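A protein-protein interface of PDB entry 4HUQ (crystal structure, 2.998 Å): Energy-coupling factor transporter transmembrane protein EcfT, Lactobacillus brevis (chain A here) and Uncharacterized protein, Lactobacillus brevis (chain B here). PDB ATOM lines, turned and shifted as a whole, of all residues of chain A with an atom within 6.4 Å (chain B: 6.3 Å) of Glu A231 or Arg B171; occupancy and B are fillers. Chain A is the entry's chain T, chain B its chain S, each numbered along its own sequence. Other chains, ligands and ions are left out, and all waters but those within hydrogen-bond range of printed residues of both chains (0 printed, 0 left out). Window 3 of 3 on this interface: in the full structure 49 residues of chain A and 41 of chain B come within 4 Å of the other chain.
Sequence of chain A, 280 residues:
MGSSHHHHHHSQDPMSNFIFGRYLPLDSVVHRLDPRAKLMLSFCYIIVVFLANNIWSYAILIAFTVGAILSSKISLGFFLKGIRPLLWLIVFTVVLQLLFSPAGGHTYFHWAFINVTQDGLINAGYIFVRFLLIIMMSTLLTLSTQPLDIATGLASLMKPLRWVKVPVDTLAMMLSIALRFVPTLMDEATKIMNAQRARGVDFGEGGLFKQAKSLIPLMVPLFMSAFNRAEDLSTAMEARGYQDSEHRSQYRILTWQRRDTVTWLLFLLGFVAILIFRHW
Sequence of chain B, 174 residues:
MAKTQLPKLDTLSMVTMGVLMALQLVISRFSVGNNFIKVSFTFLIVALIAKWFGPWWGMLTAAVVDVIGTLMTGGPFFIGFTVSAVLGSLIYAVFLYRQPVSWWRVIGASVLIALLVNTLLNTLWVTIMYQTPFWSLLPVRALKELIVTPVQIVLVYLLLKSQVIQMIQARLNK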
ATOM      1  N   MET A 224      21.069 -18.286  30.336  1.00  0.00           N
ATOM      2  CA  MET A 224      21.635 -18.344  28.997  1.00  0.00           C
ATOM      3  C   MET A 224      20.788 -19.190  28.076  1.00  0.00           C
ATOM      4  O   MET A 224      20.496 -18.772  26.965  1.00  0.00           O
ATOM      5  CB  MET A 224      23.072 -18.845  29.012  1.00  0.00           C
ATOM      6  CG  MET A 224      24.077 -17.741  28.672  1.00  0.00           C
ATOM      7  SD  MET A 224      23.863 -16.997  27.024  1.00  0.00           S
ATOM      8  CE  MET A 224      24.914 -18.059  26.022  1.00  0.00           C
ATOM      9  N   ALA A 226      17.739 -19.749  28.253  1.00  0.00           N
ATOM     10  CA  ALA A 226      16.520 -19.024  28.012  1.00  0.00           C
ATOM     11  C   ALA A 226      16.790 -17.946  26.976  1.00  0.00           C
ATOM     12  O   ALA A 226      16.156 -17.921  25.920  1.00  0.00           O
ATOM     13  CB  ALA A 226      16.023 -18.424  29.296  1.00  0.00           C
ATOM     14  N   PHE A 227      17.738 -17.063  27.253  1.00  0.00           N
ATOM     15  CA  PHE A 227      18.025 -16.031  26.272  1.00  0.00           C
ATOM     16  C   PHE A 227      18.432 -16.596  24.906  1.00  0.00           C
ATOM     17  O   PHE A 227      18.082 -16.021  23.886  1.00  0.00           O
ATOM     18  CB  PHE A 227      19.050 -15.016  26.760  1.00  0.00           C
ATOM     19  CG  PHE A 227      19.412 -14.004  25.717  1.00  0.00           C
ATOM     20  CD1 PHE A 227      18.506 -13.018  25.350  1.00  0.00           C
ATOM     21  CD2 PHE A 227      20.641 -14.061  25.063  1.00  0.00           C
ATOM     22  CE1 PHE A 227      18.832 -12.093  24.365  1.00  0.00           C
ATOM     23  CE2 PHE A 227      20.975 -13.138  24.074  1.00  0.00           C
ATOM     24  CZ  PHE A 227      20.072 -12.154  23.728  1.00  0.00           C
ATOM     25  N   ASN A 228      19.152 -17.715  24.870  1.00  0.00           N
ATOM     26  CA  ASN A 228      19.452 -18.339  23.582  1.00  0.00           C
ATOM     27  C   ASN A 228      18.165 -18.784  22.913  1.00  0.00           C
ATOM     28  O   ASN A 228      17.930 -18.479  21.744  1.00  0.00           O
ATOM     29  CB  ASN A 228      20.395 -19.533  23.719  1.00  0.00           C
ATOM     30  CG  ASN A 228      21.841 -19.125  23.979  1.00  0.00           C
ATOM     31  OD1 ASN A 228      22.295 -18.072  23.526  1.00  0.00           O
ATOM     32  ND2 ASN A 228      22.577 -19.976  24.708  1.00  0.00           N
ATOM     33  N   ARG A 229      17.327 -19.497  23.662  1.00  0.00           N
ATOM     34  CA  ARG A 229      16.024 -19.924  23.158  1.00  0.00           C
ATOM     35  C   ARG A 229      15.203 -18.748  22.662  1.00  0.00           C
ATOM     36  O   ARG A 229      14.549 -18.842  21.626  1.00  0.00           O
ATOM     37  CB  ARG A 229      15.253 -20.723  24.215  1.00  0.00           C
ATOM     38  CG  ARG A 229      15.805 -22.115  24.393  1.00  0.00           C
ATOM     39  CD  ARG A 229      15.279 -22.839  25.620  1.00  0.00           C
ATOM     40  NE  ARG A 229      16.194 -23.923  25.935  1.00  0.00           N
ATOM     41  CZ  ARG A 229      16.229 -25.087  25.296  1.00  0.00           C
ATOM     42  NH1 ARG A 229      15.366 -25.339  24.323  1.00  0.00           N
ATOM     43  NH2 ARG A 229      17.127 -26.005  25.642  1.00  0.00           N
ATOM     44  N   ALA A 230      15.250 -17.643  23.400  1.00  0.00           N
ATOM     45  CA  ALA A 230      14.556 -16.423  22.994  1.00  0.00           C
ATOM     46  C   ALA A 230      14.956 -16.028  21.592  1.00  0.00           C
ATOM     47  O   ALA A 230      14.103 -15.888  20.719  1.00  0.00           O
ATOM     48  CB  ALA A 230      14.845 -15.282  23.956  1.00  0.00           C
ATOM     49  N   GLU A 231      16.261 -15.862  21.389  1.00  0.00           N
ATOM     50  CA  GLU A 231      16.778 -15.362  20.121  1.00  0.00           C
ATOM     51  C   GLU A 231      16.341 -16.267  18.990  1.00  0.00           C
ATOM     52  O   GLU A 231      15.738 -15.803  18.028  1.00  0.00           O
ATOM     53  CB  GLU A 231      18.303 -15.227  20.149  1.00  0.00           C
ATOM     54  CG  GLU A 231      18.875 -14.555  18.907  1.00  0.00           C
ATOM     55  CD  GLU A 231      20.103 -13.721  19.218  1.00  0.00           C
ATOM     56  OE1 GLU A 231      20.599 -13.806  20.362  1.00  0.00           O
ATOM     57  OE2 GLU A 231      20.568 -12.977  18.326  1.00  0.00           O
ATOM     58  N   ASP A 232      16.613 -17.561  19.140  1.00  0.00           N
ATOM     59  CA  ASP A 232      16.230 -18.554  18.143  1.00  0.00           C
ATOM     60  C   ASP A 232      14.738 -18.471  17.813  1.00  0.00           C
ATOM     61  O   ASP A 232      14.347 -18.574  16.657  1.00  0.00           O
ATOM     62  CB  ASP A 232      16.613 -19.978  18.589  1.00  0.00           C
ATOM     63  CG  ASP A 232      18.100 -20.288  18.386  1.00  0.00           C
ATOM     64  OD1 ASP A 232      18.935 -19.376  18.563  1.00  0.00           O
ATOM     65  OD2 ASP A 232      18.434 -21.451  18.052  1.00  0.00           O
ATOM     66  N   LEU A 233      13.903 -18.261  18.821  1.00  0.00           N
ATOM     67  CA  LEU A 233      12.465 -18.216  18.569  1.00  0.00           C
ATOM     68  C   LEU A 233      12.039 -16.960  17.818  1.00  0.00           C
ATOM     69  O   LEU A 233      11.204 -17.017  16.920  1.00  0.00           O
ATOM     70  CB  LEU A 233      11.672 -18.332  19.864  1.00  0.00           C
ATOM     71  CG  LEU A 233      10.162 -18.145  19.674  1.00  0.00           C
ATOM     72  CD1 LEU A 233       9.555 -19.223  18.778  1.00  0.00           C
ATOM     73  CD2 LEU A 233       9.450 -18.082  21.012  1.00  0.00           C
ATOM     74  N   SER A 234      12.612 -15.827  18.199  1.00  0.00           N
ATOM     75  CA  SER A 234      12.261 -14.555  17.597  1.00  0.00           C
ATOM     76  C   SER A 234      12.555 -14.566  16.100  1.00  0.00           C
ATOM     77  O   SER A 234      11.694 -14.211  15.292  1.00  0.00           O
ATOM     78  CB  SER A 234      13.042 -13.436  18.277  1.00  0.00           C
ATOM     79  OG  SER A 234      13.260 -12.370  17.379  1.00  0.00           O
ATOM     80  N   THR A 235      13.770 -14.984  15.735  1.00  0.00           N
ATOM     81  CA  THR A 235      14.159 -15.021  14.327  1.00  0.00           C
ATOM     82  C   THR A 235      13.208 -15.918  13.552  1.00  0.00           C
ATOM     83  O   THR A 235      12.711 -15.538  12.491  1.00  0.00           O
ATOM     84  CB  THR A 235      15.641 -15.447  14.111  1.00  0.00           C
ATOM     85  OG1 THR A 235      15.791 -16.091  12.834  1.00  0.00           O
ATOM     86  CG2 THR A 235      16.061 -16.401  15.155  1.00  0.00           C
ATOM     87  N   ALA A 236      12.919 -17.084  14.114  1.00  0.00           N
ATOM     88  CA  ALA A 236      12.031 -18.043  13.480  1.00  0.00           C
ATOM     89  C   ALA A 236      10.652 -17.430  13.316  1.00  0.00           C
ATOM     90  O   ALA A 236       9.980 -17.650  12.310  1.00  0.00           O
ATOM     91  CB  ALA A 236      11.952 -19.319  14.301  1.00  0.00           C
ATOM     92  N   LEU B  12      12.632  -9.209  19.441  1.00  0.00           N
ATOM     93  CA  LEU B  12      13.620  -9.891  20.260  1.00  0.00           C
ATOM     94  C   LEU B  12      13.452  -9.447  21.705  1.00  0.00           C
ATOM     95  O   LEU B  12      13.489 -10.262  22.625  1.00  0.00           O
ATOM     96  CB  LEU B  12      15.033  -9.576  19.773  1.00  0.00           C
ATOM     97  CG  LEU B  12      16.179  -9.978  20.701  1.00  0.00           C
ATOM     98  CD1 LEU B  12      16.432 -11.476  20.628  1.00  0.00           C
ATOM     99  CD2 LEU B  12      17.442  -9.204  20.359  1.00  0.00           C
ATOM    100  N   VAL B  15      10.096 -10.972  22.703  1.00  0.00           N
ATOM    101  CA  VAL B  15      10.237 -12.399  23.001  1.00  0.00           C
ATOM    102  C   VAL B  15      11.025 -12.700  24.276  1.00  0.00           C
ATOM    103  O   VAL B  15      10.648 -13.564  25.071  1.00  0.00           O
ATOM    104  CB  VAL B  15      10.865 -13.168  21.825  1.00  0.00           C
ATOM    105  CG1 VAL B  15      10.899 -14.657  22.129  1.00  0.00           C
ATOM    106  CG2 VAL B  15      10.086 -12.905  20.547  1.00  0.00           C
ATOM    107  N   GLN B 166      25.577  -9.317  31.626  1.00  0.00           N
ATOM    108  CA  GLN B 166      26.344  -8.387  30.806  1.00  0.00           C
ATOM    109  C   GLN B 166      26.482  -8.897  29.383  1.00  0.00           C
ATOM    110  O   GLN B 166      26.269  -8.151  28.420  1.00  0.00           O
ATOM    111  CB  GLN B 166      27.730  -8.199  31.404  1.00  0.00           C
ATOM    112  CG  GLN B 166      27.746  -7.430  32.708  1.00  0.00           C
ATOM    113  CD  GLN B 166      27.749  -5.934  32.492  1.00  0.00           C
ATOM    114  OE1 GLN B 166      27.546  -5.449  31.372  1.00  0.00           O
ATOM    115  NE2 GLN B 166      27.992  -5.189  33.563  1.00  0.00           N
ATOM    116  N   MET B 167      26.851 -10.172  29.270  1.00  0.00           N
ATOM    117  CA  MET B 167      26.985 -10.851  27.986  1.00  0.00           C
ATOM    118  C   MET B 167      25.726 -10.643  27.125  1.00  0.00           C
ATOM    119  O   MET B 167      25.793 -10.173  25.981  1.00  0.00           O
ATOM    120  CB  MET B 167      27.243 -12.347  28.226  1.00  0.00           C
ATOM    121  CG  MET B 167      28.085 -13.046  27.161  1.00  0.00           C
ATOM    122  SD  MET B 167      29.577 -13.822  27.831  1.00  0.00           S
ATOM    123  CE  MET B 167      30.482 -12.419  28.493  1.00  0.00           C
ATOM    124  N   ILE B 168      24.583 -10.984  27.706  1.00  0.00           N
ATOM    125  CA  ILE B 168      23.292 -10.847  27.052  1.00  0.00           C
ATOM    126  C   ILE B 168      22.912  -9.392  26.796  1.00  0.00           C
ATOM    127  O   ILE B 168      22.391  -9.047  25.730  1.00  0.00           O
ATOM    128  CB  ILE B 168      22.204 -11.477  27.929  1.00  0.00           C
ATOM    129  CG1 ILE B 168      22.423 -12.993  28.006  1.00  0.00           C
ATOM    130  CG2 ILE B 168      20.801 -11.078  27.424  1.00  0.00           C
ATOM    131  CD1 ILE B 168      21.474 -13.715  28.942  1.00  0.00           C
ATOM    132  N   GLN B 169      23.169  -8.555  27.797  1.00  0.00           N
ATOM    133  CA  GLN B 169      22.836  -7.139  27.748  1.00  0.00           C
ATOM    134  C   GLN B 169      23.421  -6.550  26.495  1.00  0.00           C
ATOM    135  O   GLN B 169      22.796  -5.735  25.829  1.00  0.00           O
ATOM    136  CB  GLN B 169      23.414  -6.420  28.962  1.00  0.00           C
ATOM    137  CG  GLN B 169      22.877  -5.026  29.180  1.00  0.00           C
ATOM    138  CD  GLN B 169      23.024  -4.575  30.625  1.00  0.00           C
ATOM    139  OE1 GLN B 169      22.298  -5.038  31.511  1.00  0.00           O
ATOM    140  NE2 GLN B 169      23.970  -3.672  30.872  1.00  0.00           N
ATOM    141  N   ALA B 170      24.632  -6.983  26.176  1.00  0.00           N
ATOM    142  CA  ALA B 170      25.299  -6.537  24.973  1.00  0.00           C
ATOM    143  C   ALA B 170      24.521  -7.009  23.765  1.00  0.00           C
ATOM    144  O   ALA B 170      24.252  -6.238  22.848  1.00  0.00           O
ATOM    145  CB  ALA B 170      26.703  -7.079  24.934  1.00  0.00           C
ATOM    146  N   ARG B 171      24.143  -8.279  23.785  1.00  0.00           N
ATOM    147  CA  ARG B 171      23.473  -8.904  22.655  1.00  0.00           C
ATOM    148  C   ARG B 171      22.125  -8.279  22.346  1.00  0.00           C
ATOM    149  O   ARG B 171      21.664  -8.329  21.213  1.00  0.00           O
ATOM    150  CB  ARG B 171      23.307 -10.397  22.900  1.00  0.00           C
ATOM    151  CG  ARG B 171      24.585 -11.170  22.720  1.00  0.00           C
ATOM    152  CD  ARG B 171      24.321 -12.431  21.930  1.00  0.00           C
ATOM    153  NE  ARG B 171      24.177 -13.594  22.799  1.00  0.00           N
ATOM    154  CZ  ARG B 171      23.542 -14.704  22.447  1.00  0.00           C
ATOM    155  NH1 ARG B 171      22.988 -14.790  21.243  1.00  0.00           N
ATOM    156  NH2 ARG B 171      23.458 -15.724  23.294  1.00  0.00           N
ATOM    157  N   LEU B 172      21.498  -7.688  23.355  1.00  0.00           N
ATOM    158  CA  LEU B 172      20.223  -7.004  23.167  1.00  0.00           C
ATOM    159  C   LEU B 172      20.392  -5.593  22.602  1.00  0.00           C
ATOM    160  O   LEU B 172      19.492  -5.074  21.942  1.00  0.00           O
ATOM    161  CB  LEU B 172      19.446  -6.957  24.481  1.00  0.00           C
ATOM    162  CG  LEU B 172      18.788  -8.269  24.909  1.00  0.00           C
ATOM    163  CD1 LEU B 172      18.342  -8.217  26.372  1.00  0.00           C
ATOM    164  CD2 LEU B 172      17.610  -8.575  23.999  1.00  0.00           C
ATOM    165  N   ASN B 173      21.541  -4.977  22.872  1.00  0.00           N
ATOM    166  CA  ASN B 173      21.851  -3.657  22.328  1.00  0.00           C
ATOM    167  C   ASN B 173      22.511  -3.756  20.948  1.00  0.00           C
ATOM    168  O   ASN B 173      23.503  -4.474  20.750  1.00  0.00           O
ATOM    169  CB  ASN B 173      22.753  -2.868  23.284  1.00  0.00           C
ATOM    170  CG  ASN B 173      22.188  -2.777  24.705  1.00  0.00           C
ATOM    171  OD1 ASN B 173      21.100  -3.283  25.004  1.00  0.00           O
ATOM    172  ND2 ASN B 173      22.942  -2.140  25.593  1.00  0.00           N
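NH1 of Arg B171 is in salt-bridge range of OE1 of Glu A231, 2.7 Å away.
The guanidinium group of Arg B171 is in hydrogen-bond range of the side-chain amide oxygen of Asn A228, at 2.6 Å.
The backbone carbonyl oxygen (O) of Met A224 sits close to the side-chain amide nitrogen (ND2) of Asn A228 (3.3 Å).
Among the printed residues, merely in contact across the chains: Met A224 with Arg B171, Phe A227 with Ile B168, Phe A227 with Arg B171, Phe A227 with Leu B172, Ala A230 with Val B15, Glu A231 with Leu B12, Leu A233 with Val B15, Ser A234 with Leu B12 and Ser A234 with Val B15.
Printed residues of chain B within 4 Å of Met A224: Arg B171.
Printed residues of chain B within 4 Å of Ala A230: Val B15.
Of chain B, only Leu B12 (3.9 Å) and Arg B171 (2.7 Å) come within 4 Å of Glu A231.
Of the printed residues of chain B, Leu A233 touches Val B15.
Of the printed residues of chain A, Val B15 touches Ala A230 (3.7 Å), Leu A233 (3.9 Å) and Ser A234 (3.8 Å).
Of chain A, only Met A224, Phe A227, Asn A228 and Glu A231 come within 4 Å of Arg B171.
Of the printed residues of chain A, Leu B172 touches Phe A227.
The nearest printed residue of chain A that does not touch Val B15 is Glu A231 (5.5 Å).
Hydrophobic or aromatic side chains of chain A that line the printed part of chain B: Met A224, Phe A227 and Leu A233.
Of the 10 printed residues of chain B, 5 touch a printed residue of chain A.
Printed residues of chain B that touch a printed residue of chain A: Leu B12, Val B15, Ile B168, Arg B171 and Leu B172.
Hydrophobic or aromatic side chains of chain B that line the printed part of chain A: Leu B12, Val B15, Ile B168 and Leu B172.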
